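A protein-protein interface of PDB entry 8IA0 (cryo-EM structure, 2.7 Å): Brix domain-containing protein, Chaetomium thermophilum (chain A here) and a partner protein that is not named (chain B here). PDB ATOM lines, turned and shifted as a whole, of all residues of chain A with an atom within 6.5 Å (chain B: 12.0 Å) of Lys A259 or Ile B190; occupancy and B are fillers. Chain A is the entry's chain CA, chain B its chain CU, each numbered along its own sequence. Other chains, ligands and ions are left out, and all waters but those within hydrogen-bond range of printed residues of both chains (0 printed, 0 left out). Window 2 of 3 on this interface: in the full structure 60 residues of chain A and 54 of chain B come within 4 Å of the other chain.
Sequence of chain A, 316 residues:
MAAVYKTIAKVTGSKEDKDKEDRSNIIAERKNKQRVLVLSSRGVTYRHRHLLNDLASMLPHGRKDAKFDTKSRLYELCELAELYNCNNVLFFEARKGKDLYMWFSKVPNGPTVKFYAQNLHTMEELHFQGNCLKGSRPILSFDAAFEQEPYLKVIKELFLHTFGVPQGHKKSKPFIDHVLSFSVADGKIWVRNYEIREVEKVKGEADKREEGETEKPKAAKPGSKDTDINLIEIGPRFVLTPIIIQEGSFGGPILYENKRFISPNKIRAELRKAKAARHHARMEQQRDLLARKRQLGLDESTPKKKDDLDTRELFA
N of Glu A257 is in hydrogen-bond range of O of Ile B190 (3.1 Å).
The backbone NH (N) of Asn B192 lies within hydrogen-bond range of the backbone carbonyl oxygen (O) of Leu A255 (3.1 Å).
The side-chain amino group (NZ) of Lys A259 sits close to the backbone NH (N) of Ile B190, at 3.1 Å.
The side-chain amino group (NZ) of Lys B193 sits close to the side-chain amide nitrogen (ND2) of Asn B191 (3.2 Å).
The side-chain amide oxygen (OD1) of Asn B192 lies close to the side-chain carboxylate (OE1) of Glu B194, 3.2 Å away.
N of Gly B195 is in hydrogen-bond range of OD1 of Asn B192 (3.0 Å).
The backbone carbonyl oxygen (O) of Ile A245 sits at hydrogen-bond distance from the backbone NH (N) of Leu A255, 2.8 Å away.
N of Ile A245 is in hydrogen-bond range of O of Tyr A256, 3.3 Å away.
Among the printed residues, pairs that only touch across the chains: Ile A245 with Leu B196 (3.99 Å), Ile A254 with Ile B190 (3.4 Å), Leu A255 with Ile B190 (3.7 Å), Leu A255 with Asn B191 (3.8 Å), Leu A255 with Gly B195 (3.7 Å), Leu A255 with Leu B196 (3.7 Å), Tyr A256 with Ile B190 (3.3 Å) and Tyr A256 with Asn B191 (3.9 Å).
Ile A254 touches one residue of chain B.
Printed residues of chain B within 4 Å of Leu A255: Ile B190 (3.7 Å), Asn B191 (3.8 Å), Asn B192 (3.1 Å), Gly B195 (3.7 Å) and Leu B196 (3.7 Å).
Tyr A256 touches just these residues of chain B: Ile B190 (3.3 Å) and Asn B191 (3.9 Å).
Asn A258 touches none of the printed residues of chain B.
Printed residues of chain B within 4 Å of Lys A259: Ile B190 (3.1 Å).
No residue of chain B comes within 4 Å of Arg A260.
Of chain A, only Ile A254, Leu A255, Tyr A256, Glu A257 and Lys A259 come within 4 Å of Ile B190.
Of the printed residues of chain A, Asn B191 touches Leu A255 and Tyr A256.
Printed residues of chain A within 4 Å of Asn B192: Leu A255 (3.1 Å).
Of the printed residues of chain A, Gly B195 touches Leu A255.
Of the printed residues of chain A, Leu B196 touches Ile A245 and Leu A255.
Leu B197 touches none of the printed residues of chain A.
The nearest printed residue of chain B that does not touch Leu A255 is Lys B193 (5.5 Å).
Hydrophobic or aromatic side chains of chain A within 4 Å of the printed part of chain B: Ile A245, Leu A255 and Tyr A256.
Hydrophobic or aromatic side chains of chain B within 4 Å of the printed part of chain A: Ile B190 and Leu B196.
Among the printed residues, 11 pairs touch across the chains.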
ATOM      1  N   ILE A 243     -26.650 -14.683  16.335  1.00  0.00           N
ATOM      2  CA  ILE A 243     -26.220 -14.582  17.725  1.00  0.00           C
ATOM      3  C   ILE A 243     -24.797 -15.093  17.887  1.00  0.00           C
ATOM      4  O   ILE A 243     -23.938 -14.406  18.450  1.00  0.00           O
ATOM      5  CB  ILE A 243     -27.192 -15.341  18.645  1.00  0.00           C
ATOM      6  CG1 ILE A 243     -28.545 -14.638  18.693  1.00  0.00           C
ATOM      7  CG2 ILE A 243     -26.613 -15.467  20.041  1.00  0.00           C
ATOM      8  CD1 ILE A 243     -29.617 -15.455  19.354  1.00  0.00           C
ATOM      9  N   ILE A 245     -21.662 -18.147  16.293  1.00  0.00           N
ATOM     10  CA  ILE A 245     -21.179 -19.184  15.389  1.00  0.00           C
ATOM     11  C   ILE A 245     -20.135 -19.997  16.137  1.00  0.00           C
ATOM     12  O   ILE A 245     -19.175 -19.434  16.676  1.00  0.00           O
ATOM     13  CB  ILE A 245     -20.576 -18.594  14.100  1.00  0.00           C
ATOM     14  CG1 ILE A 245     -21.658 -17.928  13.252  1.00  0.00           C
ATOM     15  CG2 ILE A 245     -19.866 -19.672  13.304  1.00  0.00           C
ATOM     16  CD1 ILE A 245     -21.138 -17.358  11.954  1.00  0.00           C
ATOM     17  N   ILE A 254     -16.211 -20.631  20.267  1.00  0.00           N
ATOM     18  CA  ILE A 254     -17.041 -19.608  19.648  1.00  0.00           C
ATOM     19  C   ILE A 254     -16.184 -18.809  18.680  1.00  0.00           C
ATOM     20  O   ILE A 254     -15.141 -18.265  19.062  1.00  0.00           O
ATOM     21  CB  ILE A 254     -17.673 -18.696  20.711  1.00  0.00           C
ATOM     22  CG1 ILE A 254     -18.690 -19.479  21.543  1.00  0.00           C
ATOM     23  CG2 ILE A 254     -18.290 -17.472  20.061  1.00  0.00           C
ATOM     24  CD1 ILE A 254     -19.615 -20.345  20.723  1.00  0.00           C
ATOM     25  N   LEU A 255     -16.621 -18.735  17.425  1.00  0.00           N
ATOM     26  CA  LEU A 255     -15.891 -17.997  16.407  1.00  0.00           C
ATOM     27  C   LEU A 255     -16.498 -16.639  16.094  1.00  0.00           C
ATOM     28  O   LEU A 255     -15.844 -15.824  15.436  1.00  0.00           O
ATOM     29  CB  LEU A 255     -15.805 -18.820  15.116  1.00  0.00           C
ATOM     30  CG  LEU A 255     -15.223 -20.225  15.257  1.00  0.00           C
ATOM     31  CD1 LEU A 255     -15.165 -20.909  13.904  1.00  0.00           C
ATOM     32  CD2 LEU A 255     -13.848 -20.182  15.901  1.00  0.00           C
ATOM     33  N   TYR A 256     -17.722 -16.375  16.544  1.00  0.00           N
ATOM     34  CA  TYR A 256     -18.343 -15.074  16.353  1.00  0.00           C
ATOM     35  C   TYR A 256     -19.354 -14.827  17.461  1.00  0.00           C
ATOM     36  O   TYR A 256     -20.098 -15.729  17.846  1.00  0.00           O
ATOM     37  CB  TYR A 256     -19.033 -14.967  14.990  1.00  0.00           C
ATOM     38  CG  TYR A 256     -19.697 -13.631  14.761  1.00  0.00           C
ATOM     39  CD1 TYR A 256     -18.947 -12.468  14.682  1.00  0.00           C
ATOM     40  CD2 TYR A 256     -21.075 -13.531  14.639  1.00  0.00           C
ATOM     41  CE1 TYR A 256     -19.551 -11.244  14.478  1.00  0.00           C
ATOM     42  CE2 TYR A 256     -21.686 -12.312  14.436  1.00  0.00           C
ATOM     43  CZ  TYR A 256     -20.920 -11.173  14.356  1.00  0.00           C
ATOM     44  OH  TYR A 256     -21.525  -9.955  14.153  1.00  0.00           O
ATOM     45  N   GLU A 257     -19.368 -13.597  17.965  1.00  0.00           N
ATOM     46  CA  GLU A 257     -20.342 -13.138  18.942  1.00  0.00           C
ATOM     47  C   GLU A 257     -20.948 -11.837  18.443  1.00  0.00           C
ATOM     48  O   GLU A 257     -20.244 -11.000  17.869  1.00  0.00           O
ATOM     49  CB  GLU A 257     -19.699 -12.925  20.312  1.00  0.00           C
ATOM     50  CG  GLU A 257     -20.238 -13.822  21.409  1.00  0.00           C
ATOM     51  CD  GLU A 257     -19.667 -13.473  22.766  1.00  0.00           C
ATOM     52  OE1 GLU A 257     -19.136 -12.353  22.918  1.00  0.00           O
ATOM     53  OE2 GLU A 257     -19.741 -14.317  23.683  1.00  0.00           O
ATOM     54  N   ASN A 258     -22.252 -11.665  18.659  1.00  0.00           N
ATOM     55  CA  ASN A 258     -22.921 -10.479  18.138  1.00  0.00           C
ATOM     56  C   ASN A 258     -22.518  -9.224  18.904  1.00  0.00           C
ATOM     57  O   ASN A 258     -22.300  -8.168  18.298  1.00  0.00           O
ATOM     58  CB  ASN A 258     -24.435 -10.665  18.176  1.00  0.00           C
ATOM     59  CG  ASN A 258     -25.149  -9.809  17.152  1.00  0.00           C
ATOM     60  OD1 ASN A 258     -24.539  -8.959  16.507  1.00  0.00           O
ATOM     61  ND2 ASN A 258     -26.448 -10.026  17.000  1.00  0.00           N
ATOM     62  N   LYS A 259     -22.442  -9.315  20.234  1.00  0.00           N
ATOM     63  CA  LYS A 259     -22.039  -8.210  21.103  1.00  0.00           C
ATOM     64  C   LYS A 259     -23.014  -7.038  21.047  1.00  0.00           C
ATOM     65  O   LYS A 259     -22.802  -6.015  21.706  1.00  0.00           O
ATOM     66  CB  LYS A 259     -20.627  -7.729  20.759  1.00  0.00           C
ATOM     67  CG  LYS A 259     -19.518  -8.601  21.320  1.00  0.00           C
ATOM     68  CD  LYS A 259     -18.153  -8.027  20.982  1.00  0.00           C
ATOM     69  CE  LYS A 259     -17.042  -8.837  21.624  1.00  0.00           C
ATOM     70  NZ  LYS A 259     -15.695  -8.367  21.199  1.00  0.00           N
ATOM     71  N   ARG A 260     -24.087  -7.174  20.268  1.00  0.00           N
ATOM     72  CA  ARG A 260     -25.122  -6.155  20.177  1.00  0.00           C
ATOM     73  C   ARG A 260     -26.517  -6.759  20.242  1.00  0.00           C
ATOM     74  O   ARG A 260     -27.501  -6.039  20.046  1.00  0.00           O
ATOM     75  CB  ARG A 260     -24.969  -5.340  18.887  1.00  0.00           C
ATOM     76  CG  ARG A 260     -23.694  -4.520  18.811  1.00  0.00           C
ATOM     77  CD  ARG A 260     -23.647  -3.696  17.534  1.00  0.00           C
ATOM     78  NE  ARG A 260     -24.308  -4.372  16.425  1.00  0.00           N
ATOM     79  CZ  ARG A 260     -24.165  -4.036  15.150  1.00  0.00           C
ATOM     80  NH1 ARG A 260     -23.388  -3.030  14.784  1.00  0.00           N
ATOM     81  NH2 ARG A 260     -24.819  -4.725  14.219  1.00  0.00           N
ATOM     82  N   PHE A 261     -26.625  -8.058  20.508  1.00  0.00           N
ATOM     83  CA  PHE A 261     -27.923  -8.713  20.549  1.00  0.00           C
ATOM     84  C   PHE A 261     -28.706  -8.254  21.769  1.00  0.00           C
ATOM     85  O   PHE A 261     -28.216  -8.323  22.899  1.00  0.00           O
ATOM     86  CB  PHE A 261     -27.744 -10.230  20.572  1.00  0.00           C
ATOM     87  CG  PHE A 261     -29.029 -10.988  20.724  1.00  0.00           C
ATOM     88  CD1 PHE A 261     -30.089 -10.758  19.868  1.00  0.00           C
ATOM     89  CD2 PHE A 261     -29.178 -11.927  21.727  1.00  0.00           C
ATOM     90  CE1 PHE A 261     -31.272 -11.449  20.008  1.00  0.00           C
ATOM     91  CE2 PHE A 261     -30.359 -12.622  21.872  1.00  0.00           C
ATOM     92  CZ  PHE A 261     -31.408 -12.384  21.011  1.00  0.00           C
ATOM     93  N   ILE B 190     -15.687 -11.206  19.949  1.00  0.00           N
ATOM     94  CA  ILE B 190     -15.029 -12.358  19.355  1.00  0.00           C
ATOM     95  C   ILE B 190     -15.366 -12.397  17.869  1.00  0.00           C
ATOM     96  O   ILE B 190     -16.526 -12.560  17.484  1.00  0.00           O
ATOM     97  CB  ILE B 190     -15.433 -13.662  20.071  1.00  0.00           C
ATOM     98  CG1 ILE B 190     -14.508 -13.923  21.257  1.00  0.00           C
ATOM     99  CG2 ILE B 190     -15.352 -14.850  19.130  1.00  0.00           C
ATOM    100  CD1 ILE B 190     -15.139 -14.763  22.345  1.00  0.00           C
ATOM    101  N   ASN B 191     -14.348 -12.195  17.033  1.00  0.00           N
ATOM    102  CA  ASN B 191     -14.477 -12.307  15.578  1.00  0.00           C
ATOM    103  C   ASN B 191     -13.201 -12.985  15.085  1.00  0.00           C
ATOM    104  O   ASN B 191     -12.220 -12.317  14.752  1.00  0.00           O
ATOM    105  CB  ASN B 191     -14.690 -10.944  14.933  1.00  0.00           C
ATOM    106  CG  ASN B 191     -15.196 -11.042  13.508  1.00  0.00           C
ATOM    107  OD1 ASN B 191     -15.469 -12.131  13.006  1.00  0.00           O
ATOM    108  ND2 ASN B 191     -15.319  -9.899  12.846  1.00  0.00           N
ATOM    109  N   ASN B 192     -13.224 -14.315  15.034  1.00  0.00           N
ATOM    110  CA  ASN B 192     -12.041 -15.100  14.687  1.00  0.00           C
ATOM    111  C   ASN B 192     -12.077 -15.339  13.184  1.00  0.00           C
ATOM    112  O   ASN B 192     -12.579 -16.356  12.704  1.00  0.00           O
ATOM    113  CB  ASN B 192     -12.014 -16.403  15.477  1.00  0.00           C
ATOM    114  CG  ASN B 192     -10.664 -17.102  15.425  1.00  0.00           C
ATOM    115  OD1 ASN B 192      -9.831 -16.789  14.575  1.00  0.00           O
ATOM    116  ND2 ASN B 192     -10.448 -18.058  16.317  1.00  0.00           N
ATOM    117  N   LYS B 193     -11.526 -14.386  12.430  1.00  0.00           N
ATOM    118  CA  LYS B 193     -11.567 -14.469  10.974  1.00  0.00           C
ATOM    119  C   LYS B 193     -10.787 -15.672  10.458  1.00  0.00           C
ATOM    120  O   LYS B 193     -11.232 -16.347   9.524  1.00  0.00           O
ATOM    121  CB  LYS B 193     -11.036 -13.175  10.363  1.00  0.00           C
ATOM    122  CG  LYS B 193     -12.101 -12.114  10.169  1.00  0.00           C
ATOM    123  CD  LYS B 193     -11.493 -10.732  10.040  1.00  0.00           C
ATOM    124  CE  LYS B 193     -12.336  -9.694  10.759  1.00  0.00           C
ATOM    125  NZ  LYS B 193     -13.657  -9.501  10.100  1.00  0.00           N
ATOM    126  N   GLU B 194      -9.621 -15.952  11.043  1.00  0.00           N
ATOM    127  CA  GLU B 194      -8.854 -17.123  10.634  1.00  0.00           C
ATOM    128  C   GLU B 194      -9.629 -18.404  10.912  1.00  0.00           C
ATOM    129  O   GLU B 194      -9.667 -19.316  10.079  1.00  0.00           O
ATOM    130  CB  GLU B 194      -7.489 -17.159  11.335  1.00  0.00           C
ATOM    131  CG  GLU B 194      -6.638 -15.869  11.342  1.00  0.00           C
ATOM    132  CD  GLU B 194      -7.265 -14.672  12.052  1.00  0.00           C
ATOM    133  OE1 GLU B 194      -8.409 -14.773  12.542  1.00  0.00           O
ATOM    134  OE2 GLU B 194      -6.598 -13.618  12.118  1.00  0.00           O
ATOM    135  N   GLY B 195     -10.256 -18.490  12.087  1.00  0.00           N
ATOM    136  CA  GLY B 195     -11.067 -19.655  12.397  1.00  0.00           C
ATOM    137  C   GLY B 195     -12.312 -19.748  11.536  1.00  0.00           C
ATOM    138  O   GLY B 195     -12.720 -20.841  11.136  1.00  0.00           O
ATOM    139  N   LEU B 196     -12.938 -18.604  11.248  1.00  0.00           N
ATOM    140  CA  LEU B 196     -14.140 -18.606  10.419  1.00  0.00           C
ATOM    141  C   LEU B 196     -13.835 -19.067   9.000  1.00  0.00           C
ATOM    142  O   LEU B 196     -14.602 -19.839   8.414  1.00  0.00           O
ATOM    143  CB  LEU B 196     -14.774 -17.216  10.410  1.00  0.00           C
ATOM    144  CG  LEU B 196     -15.582 -16.845  11.656  1.00  0.00           C
ATOM    145  CD1 LEU B 196     -15.737 -15.340  11.768  1.00  0.00           C
ATOM    146  CD2 LEU B 196     -16.940 -17.524  11.636  1.00  0.00           C
ATOM    147  N   LEU B 197     -12.723 -18.603   8.428  1.00  0.00           N
ATOM    148  CA  LEU B 197     -12.343 -19.052   7.094  1.00  0.00           C
ATOM    149  C   LEU B 197     -11.899 -20.508   7.098  1.00  0.00           C
ATOM    150  O   LEU B 197     -12.124 -21.225   6.118  1.00  0.00           O
ATOM    151  CB  LEU B 197     -11.239 -18.157   6.534  1.00  0.00           C
ATOM    152  CG  LEU B 197     -11.656 -16.732   6.170  1.00  0.00           C
ATOM    153  CD1 LEU B 197     -10.466 -15.938   5.663  1.00  0.00           C
ATOM    154  CD2 LEU B 197     -12.770 -16.749   5.141  1.00  0.00           C
